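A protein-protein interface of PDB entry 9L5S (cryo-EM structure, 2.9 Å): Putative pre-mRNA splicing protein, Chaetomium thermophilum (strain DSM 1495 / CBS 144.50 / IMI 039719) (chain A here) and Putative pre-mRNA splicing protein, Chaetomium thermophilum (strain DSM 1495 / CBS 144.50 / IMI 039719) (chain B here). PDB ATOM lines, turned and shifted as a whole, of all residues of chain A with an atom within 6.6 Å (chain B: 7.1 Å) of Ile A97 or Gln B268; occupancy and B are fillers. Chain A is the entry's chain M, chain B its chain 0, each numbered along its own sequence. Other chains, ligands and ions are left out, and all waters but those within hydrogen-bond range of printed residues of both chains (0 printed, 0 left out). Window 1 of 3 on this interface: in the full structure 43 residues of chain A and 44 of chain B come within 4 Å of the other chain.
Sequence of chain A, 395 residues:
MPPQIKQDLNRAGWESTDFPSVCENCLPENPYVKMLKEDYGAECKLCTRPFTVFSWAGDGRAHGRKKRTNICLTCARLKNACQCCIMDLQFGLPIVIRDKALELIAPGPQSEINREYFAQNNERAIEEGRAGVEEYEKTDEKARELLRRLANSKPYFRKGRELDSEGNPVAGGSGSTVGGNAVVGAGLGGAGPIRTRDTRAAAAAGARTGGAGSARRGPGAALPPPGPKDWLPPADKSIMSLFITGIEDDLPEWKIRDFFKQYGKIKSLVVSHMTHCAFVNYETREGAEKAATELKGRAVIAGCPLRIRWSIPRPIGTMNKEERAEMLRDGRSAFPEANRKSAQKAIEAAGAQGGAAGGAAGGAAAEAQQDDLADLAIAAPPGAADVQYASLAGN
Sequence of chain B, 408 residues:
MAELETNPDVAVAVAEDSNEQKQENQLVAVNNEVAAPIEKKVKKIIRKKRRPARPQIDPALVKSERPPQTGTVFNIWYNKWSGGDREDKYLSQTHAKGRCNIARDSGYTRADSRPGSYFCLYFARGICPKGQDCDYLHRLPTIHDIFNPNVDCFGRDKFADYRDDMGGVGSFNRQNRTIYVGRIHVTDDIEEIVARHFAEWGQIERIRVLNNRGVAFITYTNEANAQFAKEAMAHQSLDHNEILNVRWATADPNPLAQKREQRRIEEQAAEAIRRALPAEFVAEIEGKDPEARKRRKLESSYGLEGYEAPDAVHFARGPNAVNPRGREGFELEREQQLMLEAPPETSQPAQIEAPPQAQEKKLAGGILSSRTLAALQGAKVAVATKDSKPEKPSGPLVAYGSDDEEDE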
ATOM      1  N   LEU A  93      28.482  14.446  -1.302  1.00  0.00           N
ATOM      2  CA  LEU A  93      28.475  13.800  -2.602  1.00  0.00           C
ATOM      3  C   LEU A  93      29.843  13.921  -3.263  1.00  0.00           C
ATOM      4  O   LEU A  93      30.589  14.860  -2.977  1.00  0.00           O
ATOM      5  CB  LEU A  93      27.428  14.430  -3.527  1.00  0.00           C
ATOM      6  CG  LEU A  93      25.964  14.063  -3.312  1.00  0.00           C
ATOM      7  CD1 LEU A  93      25.075  15.189  -3.805  1.00  0.00           C
ATOM      8  CD2 LEU A  93      25.625  12.759  -4.014  1.00  0.00           C
ATOM      9  N   PRO A  94      30.201  12.985  -4.145  1.00  0.00           N
ATOM     10  CA  PRO A  94      31.397  13.180  -4.974  1.00  0.00           C
ATOM     11  C   PRO A  94      31.247  14.401  -5.868  1.00  0.00           C
ATOM     12  O   PRO A  94      30.136  14.818  -6.204  1.00  0.00           O
ATOM     13  CB  PRO A  94      31.479  11.888  -5.795  1.00  0.00           C
ATOM     14  CG  PRO A  94      30.709  10.885  -5.016  1.00  0.00           C
ATOM     15  CD  PRO A  94      29.637  11.632  -4.286  1.00  0.00           C
ATOM     16  N   ILE A  95      32.392  14.990  -6.224  1.00  0.00           N
ATOM     17  CA  ILE A  95      32.404  16.265  -6.940  1.00  0.00           C
ATOM     18  C   ILE A  95      31.764  16.123  -8.316  1.00  0.00           C
ATOM     19  O   ILE A  95      30.945  16.956  -8.725  1.00  0.00           O
ATOM     20  CB  ILE A  95      33.846  16.801  -7.033  1.00  0.00           C
ATOM     21  CG1 ILE A  95      34.353  17.214  -5.649  1.00  0.00           C
ATOM     22  CG2 ILE A  95      33.934  17.970  -8.000  1.00  0.00           C
ATOM     23  CD1 ILE A  95      33.374  18.054  -4.859  1.00  0.00           C
ATOM     24  N   VAL A  96      32.105  15.056  -9.041  1.00  0.00           N
ATOM     25  CA  VAL A  96      31.548  14.872 -10.376  1.00  0.00           C
ATOM     26  C   VAL A  96      30.067  14.514 -10.315  1.00  0.00           C
ATOM     27  O   VAL A  96      29.298  14.924 -11.190  1.00  0.00           O
ATOM     28  CB  VAL A  96      32.369  13.833 -11.163  1.00  0.00           C
ATOM     29  CG1 VAL A  96      33.744  14.397 -11.457  1.00  0.00           C
ATOM     30  CG2 VAL A  96      32.490  12.530 -10.387  1.00  0.00           C
ATOM     31  N   ILE A  97      29.638  13.773  -9.289  1.00  0.00           N
ATOM     32  CA  ILE A  97      28.219  13.455  -9.130  1.00  0.00           C
ATOM     33  C   ILE A  97      27.420  14.729  -8.889  1.00  0.00           C
ATOM     34  O   ILE A  97      26.374  14.962  -9.514  1.00  0.00           O
ATOM     35  CB  ILE A  97      28.025  12.448  -7.981  1.00  0.00           C
ATOM     36  CG1 ILE A  97      28.781  11.151  -8.270  1.00  0.00           C
ATOM     37  CG2 ILE A  97      26.547  12.172  -7.751  1.00  0.00           C
ATOM     38  CD1 ILE A  97      28.287  10.403  -9.477  1.00  0.00           C
ATOM     39  N   ARG A  98      27.929  15.584  -7.999  1.00  0.00           N
ATOM     40  CA  ARG A  98      27.303  16.869  -7.704  1.00  0.00           C
ATOM     41  C   ARG A  98      27.250  17.754  -8.945  1.00  0.00           C
ATOM     42  O   ARG A  98      26.225  18.390  -9.219  1.00  0.00           O
ATOM     43  CB  ARG A  98      28.082  17.549  -6.571  1.00  0.00           C
ATOM     44  CG  ARG A  98      27.452  18.779  -5.916  1.00  0.00           C
ATOM     45  CD  ARG A  98      27.900  20.064  -6.591  1.00  0.00           C
ATOM     46  NE  ARG A  98      29.345  20.129  -6.774  1.00  0.00           N
ATOM     47  CZ  ARG A  98      30.195  20.670  -5.913  1.00  0.00           C
ATOM     48  NH1 ARG A  98      29.775  21.266  -4.811  1.00  0.00           N
ATOM     49  NH2 ARG A  98      31.498  20.630  -6.174  1.00  0.00           N
ATOM     50  N   ASP A  99      28.342  17.795  -9.714  1.00  0.00           N
ATOM     51  CA  ASP A  99      28.398  18.673 -10.878  1.00  0.00           C
ATOM     52  C   ASP A  99      27.488  18.183 -11.999  1.00  0.00           C
ATOM     53  O   ASP A  99      26.847  18.993 -12.678  1.00  0.00           O
ATOM     54  CB  ASP A  99      29.840  18.803 -11.368  1.00  0.00           C
ATOM     55  CG  ASP A  99      30.604  19.888 -10.636  1.00  0.00           C
ATOM     56  OD1 ASP A  99      30.001  20.565  -9.776  1.00  0.00           O
ATOM     57  OD2 ASP A  99      31.807  20.067 -10.919  1.00  0.00           O
ATOM     58  N   LYS A 100      27.429  16.867 -12.223  1.00  0.00           N
ATOM     59  CA  LYS A 100      26.536  16.337 -13.249  1.00  0.00           C
ATOM     60  C   LYS A 100      25.074  16.504 -12.858  1.00  0.00           C
ATOM     61  O   LYS A 100      24.238  16.837 -13.706  1.00  0.00           O
ATOM     62  CB  LYS A 100      26.851  14.867 -13.526  1.00  0.00           C
ATOM     63  CG  LYS A 100      28.197  14.632 -14.189  1.00  0.00           C
ATOM     64  CD  LYS A 100      28.339  15.433 -15.469  1.00  0.00           C
ATOM     65  CE  LYS A 100      29.502  14.921 -16.298  1.00  0.00           C
ATOM     66  NZ  LYS A 100      30.774  14.949 -15.523  1.00  0.00           N
ATOM     67  N   ALA A 101      24.739  16.284 -11.587  1.00  0.00           N
ATOM     68  CA  ALA A 101      23.344  16.330 -11.180  1.00  0.00           C
ATOM     69  C   ALA A 101      22.857  17.726 -10.820  1.00  0.00           C
ATOM     70  O   ALA A 101      21.650  17.908 -10.627  1.00  0.00           O
ATOM     71  CB  ALA A 101      23.111  15.394  -9.994  1.00  0.00           C
ATOM     72  N   LEU A 102      23.745  18.714 -10.726  1.00  0.00           N
ATOM     73  CA  LEU A 102      23.324  20.081 -10.457  1.00  0.00           C
ATOM     74  C   LEU A 102      23.720  21.061 -11.552  1.00  0.00           C
ATOM     75  O   LEU A 102      23.358  22.240 -11.454  1.00  0.00           O
ATOM     76  CB  LEU A 102      23.877  20.574  -9.110  1.00  0.00           C
ATOM     77  CG  LEU A 102      23.186  20.160  -7.803  1.00  0.00           C
ATOM     78  CD1 LEU A 102      23.405  18.697  -7.438  1.00  0.00           C
ATOM     79  CD2 LEU A 102      23.620  21.073  -6.662  1.00  0.00           C
ATOM     80  N   LEU A 150      13.014  15.947 -10.663  1.00  0.00           N
ATOM     81  CA  LEU A 150      12.824  14.518 -10.445  1.00  0.00           C
ATOM     82  C   LEU A 150      11.451  14.188  -9.877  1.00  0.00           C
ATOM     83  O   LEU A 150      11.090  13.007  -9.821  1.00  0.00           O
ATOM     84  CB  LEU A 150      13.917  13.970  -9.526  1.00  0.00           C
ATOM     85  CG  LEU A 150      15.320  14.012 -10.132  1.00  0.00           C
ATOM     86  CD1 LEU A 150      16.356  13.577  -9.119  1.00  0.00           C
ATOM     87  CD2 LEU A 150      15.390  13.144 -11.379  1.00  0.00           C
ATOM     88  N   PHE B 172      38.906   9.059  -9.650  1.00  0.00           N
ATOM     89  CA  PHE B 172      37.778   9.494  -8.836  1.00  0.00           C
ATOM     90  C   PHE B 172      36.885  10.504  -9.543  1.00  0.00           C
ATOM     91  O   PHE B 172      35.905  10.964  -8.948  1.00  0.00           O
ATOM     92  CB  PHE B 172      38.255  10.066  -7.489  1.00  0.00           C
ATOM     93  CG  PHE B 172      39.365  11.090  -7.588  1.00  0.00           C
ATOM     94  CD1 PHE B 172      39.120  12.380  -8.042  1.00  0.00           C
ATOM     95  CD2 PHE B 172      40.646  10.773  -7.163  1.00  0.00           C
ATOM     96  CE1 PHE B 172      40.136  13.313  -8.113  1.00  0.00           C
ATOM     97  CE2 PHE B 172      41.666  11.706  -7.229  1.00  0.00           C
ATOM     98  CZ  PHE B 172      41.409  12.976  -7.705  1.00  0.00           C
ATOM     99  N   ASN B 173      37.190  10.856 -10.788  1.00  0.00           N
ATOM    100  CA  ASN B 173      36.344  11.753 -11.560  1.00  0.00           C
ATOM    101  C   ASN B 173      35.233  11.016 -12.295  1.00  0.00           C
ATOM    102  O   ASN B 173      34.494  11.639 -13.063  1.00  0.00           O
ATOM    103  CB  ASN B 173      37.188  12.556 -12.555  1.00  0.00           C
ATOM    104  CG  ASN B 173      38.013  13.631 -11.879  1.00  0.00           C
ATOM    105  OD1 ASN B 173      37.501  14.408 -11.075  1.00  0.00           O
ATOM    106  ND2 ASN B 173      39.298  13.685 -12.207  1.00  0.00           N
ATOM    107  N   ARG B 174      35.107   9.710 -12.081  1.00  0.00           N
ATOM    108  CA  ARG B 174      33.996   8.932 -12.613  1.00  0.00           C
ATOM    109  C   ARG B 174      33.694   7.820 -11.622  1.00  0.00           C
ATOM    110  O   ARG B 174      34.575   7.010 -11.318  1.00  0.00           O
ATOM    111  CB  ARG B 174      34.332   8.352 -13.990  1.00  0.00           C
ATOM    112  CG  ARG B 174      33.853   9.195 -15.160  1.00  0.00           C
ATOM    113  CD  ARG B 174      34.061   8.474 -16.483  1.00  0.00           C
ATOM    114  NE  ARG B 174      33.395   7.178 -16.508  1.00  0.00           N
ATOM    115  CZ  ARG B 174      33.952   6.057 -16.945  1.00  0.00           C
ATOM    116  NH1 ARG B 174      35.189   6.036 -17.412  1.00  0.00           N
ATOM    117  NH2 ARG B 174      33.248   4.928 -16.915  1.00  0.00           N
ATOM    118  N   GLN B 175      32.460   7.779 -11.116  1.00  0.00           N
ATOM    119  CA  GLN B 175      32.022   6.684 -10.249  1.00  0.00           C
ATOM    120  C   GLN B 175      31.768   5.469 -11.134  1.00  0.00           C
ATOM    121  O   GLN B 175      30.636   5.127 -11.484  1.00  0.00           O
ATOM    122  CB  GLN B 175      30.785   7.076  -9.451  1.00  0.00           C
ATOM    123  CG  GLN B 175      30.420   6.077  -8.360  1.00  0.00           C
ATOM    124  CD  GLN B 175      29.382   6.610  -7.394  1.00  0.00           C
ATOM    125  OE1 GLN B 175      29.198   7.821  -7.270  1.00  0.00           O
ATOM    126  NE2 GLN B 175      28.695   5.708  -6.708  1.00  0.00           N
ATOM    127  N   GLU B 261      22.526   6.442 -16.707  1.00  0.00           N
ATOM    128  CA  GLU B 261      23.573   6.867 -15.781  1.00  0.00           C
ATOM    129  C   GLU B 261      23.320   8.278 -15.261  1.00  0.00           C
ATOM    130  O   GLU B 261      23.516   8.552 -14.068  1.00  0.00           O
ATOM    131  CB  GLU B 261      24.938   6.781 -16.462  1.00  0.00           C
ATOM    132  CG  GLU B 261      26.111   6.994 -15.524  1.00  0.00           C
ATOM    133  CD  GLU B 261      26.381   5.784 -14.653  1.00  0.00           C
ATOM    134  OE1 GLU B 261      26.208   4.647 -15.142  1.00  0.00           O
ATOM    135  OE2 GLU B 261      26.764   5.968 -13.479  1.00  0.00           O
ATOM    136  N   GLN B 262      22.878   9.184 -16.142  1.00  0.00           N
ATOM    137  CA  GLN B 262      22.567  10.549 -15.729  1.00  0.00           C
ATOM    138  C   GLN B 262      21.422  10.574 -14.724  1.00  0.00           C
ATOM    139  O   GLN B 262      21.489  11.283 -13.709  1.00  0.00           O
ATOM    140  CB  GLN B 262      22.224  11.393 -16.957  1.00  0.00           C
ATOM    141  CG  GLN B 262      21.833  12.828 -16.653  1.00  0.00           C
ATOM    142  CD  GLN B 262      23.032  13.709 -16.371  1.00  0.00           C
ATOM    143  OE1 GLN B 262      24.090  13.549 -16.979  1.00  0.00           O
ATOM    144  NE2 GLN B 262      22.871  14.650 -15.448  1.00  0.00           N
ATOM    145  N   ARG B 263      20.380   9.772 -14.968  1.00  0.00           N
ATOM    146  CA  ARG B 263      19.280   9.689 -14.017  1.00  0.00           C
ATOM    147  C   ARG B 263      19.744   9.131 -12.680  1.00  0.00           C
ATOM    148  O   ARG B 263      19.477   9.742 -11.644  1.00  0.00           O
ATOM    149  CB  ARG B 263      18.138   8.852 -14.590  1.00  0.00           C
ATOM    150  CG  ARG B 263      16.846   8.984 -13.797  1.00  0.00           C
ATOM    151  CD  ARG B 263      15.644   8.508 -14.589  1.00  0.00           C
ATOM    152  NE  ARG B 263      15.218   9.497 -15.571  1.00  0.00           N
ATOM    153  CZ  ARG B 263      15.226   9.306 -16.883  1.00  0.00           C
ATOM    154  NH1 ARG B 263      15.650   8.170 -17.412  1.00  0.00           N
ATOM    155  NH2 ARG B 263      14.803  10.278 -17.684  1.00  0.00           N
ATOM    156  N   ARG B 264      20.510   8.029 -12.693  1.00  0.00           N
ATOM    157  CA  ARG B 264      20.973   7.410 -11.449  1.00  0.00           C
ATOM    158  C   ARG B 264      21.829   8.370 -10.632  1.00  0.00           C
ATOM    159  O   ARG B 264      21.717   8.421  -9.399  1.00  0.00           O
ATOM    160  CB  ARG B 264      21.753   6.134 -11.758  1.00  0.00           C
ATOM    161  CG  ARG B 264      22.036   5.268 -10.543  1.00  0.00           C
ATOM    162  CD  ARG B 264      23.020   4.162 -10.879  1.00  0.00           C
ATOM    163  NE  ARG B 264      24.299   4.694 -11.336  1.00  0.00           N
ATOM    164  CZ  ARG B 264      25.304   5.019 -10.535  1.00  0.00           C
ATOM    165  NH1 ARG B 264      25.213   4.883  -9.222  1.00  0.00           N
ATOM    166  NH2 ARG B 264      26.428   5.494 -11.063  1.00  0.00           N
ATOM    167  N   ILE B 265      22.665   9.164 -11.312  1.00  0.00           N
ATOM    168  CA  ILE B 265      23.387  10.250 -10.656  1.00  0.00           C
ATOM    169  C   ILE B 265      22.405  11.240 -10.031  1.00  0.00           C
ATOM    170  O   ILE B 265      22.601  11.708  -8.896  1.00  0.00           O
ATOM    171  CB  ILE B 265      24.328  10.928 -11.673  1.00  0.00           C
ATOM    172  CG1 ILE B 265      25.560  10.057 -11.912  1.00  0.00           C
ATOM    173  CG2 ILE B 265      24.767  12.303 -11.202  1.00  0.00           C
ATOM    174  CD1 ILE B 265      26.467  10.570 -13.008  1.00  0.00           C
ATOM    175  N   GLU B 266      21.311  11.542 -10.745  1.00  0.00           N
ATOM    176  CA  GLU B 266      20.355  12.523 -10.237  1.00  0.00           C
ATOM    177  C   GLU B 266      19.599  12.023  -9.003  1.00  0.00           C
ATOM    178  O   GLU B 266      19.429  12.784  -8.046  1.00  0.00           O
ATOM    179  CB  GLU B 266      19.387  12.949 -11.343  1.00  0.00           C
ATOM    180  CG  GLU B 266      20.009  13.927 -12.333  1.00  0.00           C
ATOM    181  CD  GLU B 266      19.264  14.000 -13.651  1.00  0.00           C
ATOM    182  OE1 GLU B 266      19.103  12.955 -14.311  1.00  0.00           O
ATOM    183  OE2 GLU B 266      18.845  15.113 -14.031  1.00  0.00           O
ATOM    184  N   GLU B 267      19.147  10.759  -8.977  1.00  0.00           N
ATOM    185  CA  GLU B 267      18.534  10.305  -7.721  1.00  0.00           C
ATOM    186  C   GLU B 267      19.550  10.024  -6.617  1.00  0.00           C
ATOM    187  O   GLU B 267      19.162  10.057  -5.446  1.00  0.00           O
ATOM    188  CB  GLU B 267      17.597   9.073  -7.794  1.00  0.00           C
ATOM    189  CG  GLU B 267      16.242   9.193  -8.533  1.00  0.00           C
ATOM    190  CD  GLU B 267      16.286   8.993 -10.014  1.00  0.00           C
ATOM    191  OE1 GLU B 267      17.358   8.675 -10.521  1.00  0.00           O
ATOM    192  OE2 GLU B 267      15.240   9.158 -10.677  1.00  0.00           O
ATOM    193  N   GLN B 268      20.825   9.777  -6.929  1.00  0.00           N
ATOM    194  CA  GLN B 268      21.818   9.720  -5.856  1.00  0.00           C
ATOM    195  C   GLN B 268      21.970  11.082  -5.182  1.00  0.00           C
ATOM    196  O   GLN B 268      21.950  11.193  -3.944  1.00  0.00           O
ATOM    197  CB  GLN B 268      23.157   9.228  -6.404  1.00  0.00           C
ATOM    198  CG  GLN B 268      24.218   9.024  -5.340  1.00  0.00           C
ATOM    199  CD  GLN B 268      25.604   8.842  -5.921  1.00  0.00           C
ATOM    200  OE1 GLN B 268      25.805   8.964  -7.129  1.00  0.00           O
ATOM    201  NE2 GLN B 268      26.569   8.542  -5.063  1.00  0.00           N
ATOM    202  N   ALA B 269      22.080  12.140  -5.991  1.00  0.00           N
ATOM    203  CA  ALA B 269      22.139  13.487  -5.433  1.00  0.00           C
ATOM    204  C   ALA B 269      20.835  13.857  -4.735  1.00  0.00           C
ATOM    205  O   ALA B 269      20.848  14.549  -3.713  1.00  0.00           O
ATOM    206  CB  ALA B 269      22.465  14.500  -6.527  1.00  0.00           C
ATOM    207  N   ALA B 270      19.701  13.395  -5.269  1.00  0.00           N
ATOM    208  CA  ALA B 270      18.411  13.652  -4.638  1.00  0.00           C
ATOM    209  C   ALA B 270      18.305  12.961  -3.286  1.00  0.00           C
ATOM    210  O   ALA B 270      17.727  13.518  -2.349  1.00  0.00           O
ATOM    211  CB  ALA B 270      17.278  13.204  -5.558  1.00  0.00           C
ATOM    212  N   GLU B 271      18.843  11.743  -3.173  1.00  0.00           N
ATOM    213  CA  GLU B 271      18.896  11.059  -1.885  1.00  0.00           C
ATOM    214  C   GLU B 271      19.740  11.839  -0.889  1.00  0.00           C
ATOM    215  O   GLU B 271      19.363  11.979   0.284  1.00  0.00           O
ATOM    216  CB  GLU B 271      19.458   9.649  -2.065  1.00  0.00           C
ATOM    217  CG  GLU B 271      18.419   8.592  -2.390  1.00  0.00           C
ATOM    218  CD  GLU B 271      19.004   7.192  -2.395  1.00  0.00           C
ATOM    219  OE1 GLU B 271      20.242   7.065  -2.297  1.00  0.00           O
ATOM    220  OE2 GLU B 271      18.226   6.220  -2.500  1.00  0.00           O
ATOM    221  N   ALA B 272      20.883  12.367  -1.342  1.00  0.00           N
ATOM    222  CA  ALA B 272      21.719  13.178  -0.456  1.00  0.00           C
ATOM    223  C   ALA B 272      21.005  14.453  -0.010  1.00  0.00           C
ATOM    224  O   ALA B 272      21.076  14.836   1.166  1.00  0.00           O
ATOM    225  CB  ALA B 272      23.037  13.517  -1.147  1.00  0.00           C
ATOM    226  N   ILE B 273      20.304  15.120  -0.931  1.00  0.00           N
ATOM    227  CA  ILE B 273      19.588  16.351  -0.594  1.00  0.00           C
ATOM    228  C   ILE B 273      18.422  16.060   0.348  1.00  0.00           C
ATOM    229  O   ILE B 273      18.168  16.816   1.295  1.00  0.00           O
ATOM    230  CB  ILE B 273      19.132  17.073  -1.878  1.00  0.00           C
ATOM    231  CG1 ILE B 273      20.342  17.564  -2.675  1.00  0.00           C
ATOM    232  CG2 ILE B 273      18.232  18.254  -1.565  1.00  0.00           C
ATOM    233  CD1 ILE B 273      20.085  17.680  -4.162  1.00  0.00           C
ATOM    234  N   ARG B 274      17.707  14.952   0.119  1.00  0.00           N
ATOM    235  CA  ARG B 274      16.624  14.550   1.011  1.00  0.00           C
ATOM    236  C   ARG B 274      17.140  14.200   2.400  1.00  0.00           C
ATOM    237  O   ARG B 274      16.443  14.437   3.394  1.00  0.00           O
ATOM    238  CB  ARG B 274      15.864  13.363   0.420  1.00  0.00           C
ATOM    239  CG  ARG B 274      14.923  13.719  -0.718  1.00  0.00           C
ATOM    240  CD  ARG B 274      14.097  12.514  -1.138  1.00  0.00           C
ATOM    241  NE  ARG B 274      13.706  12.585  -2.541  1.00  0.00           N
ATOM    242  CZ  ARG B 274      14.274  11.881  -3.511  1.00  0.00           C
ATOM    243  NH1 ARG B 274      15.265  11.039  -3.266  1.00  0.00           N
ATOM    244  NH2 ARG B 274      13.836  12.025  -4.759  1.00  0.00           N
ATOM    245  N   ARG B 275      18.341  13.622   2.489  1.00  0.00           N
ATOM    246  CA  ARG B 275      18.971  13.451   3.792  1.00  0.00           C
ATOM    247  C   ARG B 275      19.324  14.792   4.423  1.00  0.00           C
ATOM    248  O   ARG B 275      19.230  14.944   5.646  1.00  0.00           O
ATOM    249  CB  ARG B 275      20.224  12.585   3.674  1.00  0.00           C
ATOM    250  CG  ARG B 275      19.975  11.097   3.838  1.00  0.00           C
ATOM    251  CD  ARG B 275      21.257  10.306   3.634  1.00  0.00           C
ATOM    252  NE  ARG B 275      21.755  10.395   2.268  1.00  0.00           N
ATOM    253  CZ  ARG B 275      22.935   9.935   1.873  1.00  0.00           C
ATOM    254  NH1 ARG B 275      23.764   9.345   2.718  1.00  0.00           N
ATOM    255  NH2 ARG B 275      23.291  10.071   0.599  1.00  0.00           N
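O of Lys A100 lies within hydrogen-bond range of NE2 of Gln B262.
Among the printed residues, merely in contact across the chains: Leu A93 with Gln B268, Leu A93 with Ala B269, Leu A93 with Ala B272, Val A96 with Asn B173, Ile A97 with Gln B175, Ile A97 with Ile B265, Ile A97 with Gln B268, Ala A101 with Ile B265, Ala A101 with Glu B266, Ala A101 with Ala B269, Leu A150 with Glu B266, Leu A150 with Glu B267 and Leu A150 with Ala B270.
Of the 19 printed residues of chain B, 10 touch a printed residue of chain A.
Hydrophobic or aromatic side chains of chain B that line the printed part of chain A: Ile B265, Ala B269, Ala B270 and Ala B272.
Printed residues of chain A that touch a printed residue of chain B: Leu A93, Val A96, Ile A97, Lys A100, Ala A101 and Leu A150.
Hydrophobic or aromatic side chains of chain A that line the printed part of chain B: Leu A93, Val A96, Ile A97, Ala A101 and Leu A150.
Among the printed residues, 14 pairs touch across the chains.
Among the printed residues, no Asp or Glu carboxylate lies within 4 Å of a Lys or Arg side-chain nitrogen of the other chain.
Ile A97 touches just these residues of chain B: Gln B175, Ile B265 and Gln B268.
Printed residues of chain A within 4 Å of Gln B262: Lys A100.
Arg B264 touches none of the printed residues of chain A.
Of the printed residues of chain A, Glu B266 touches Ala A101 (3.99 Å) and Leu A150 (3.4 Å).
Of the printed residues of chain A, Gln B268 touches Leu A93 (3.995 Å) and Ile A97 (3.4 Å).
Printed residues of chain A within 4 Å of Ala B269: Leu A93 and Ala A101.
Arg B274 touches none of the printed residues of chain A.
The nearest residue of chain B that does not touch Ile A97 is Ala B269 (4.8 Å).
The nearest printed residue of chain A that does not touch Gln B268 is Pro A94 (4.4 Å).
The nearest printed residue of chain A that does not touch Asn B173 is Lys A100 (5.6 Å).
O of Arg B263 lies close to OE1 of Glu B267 (2.6 Å).
The backbone NH of Arg B263 sits close to the side-chain carboxylate of Glu B266 (3.5 Å).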
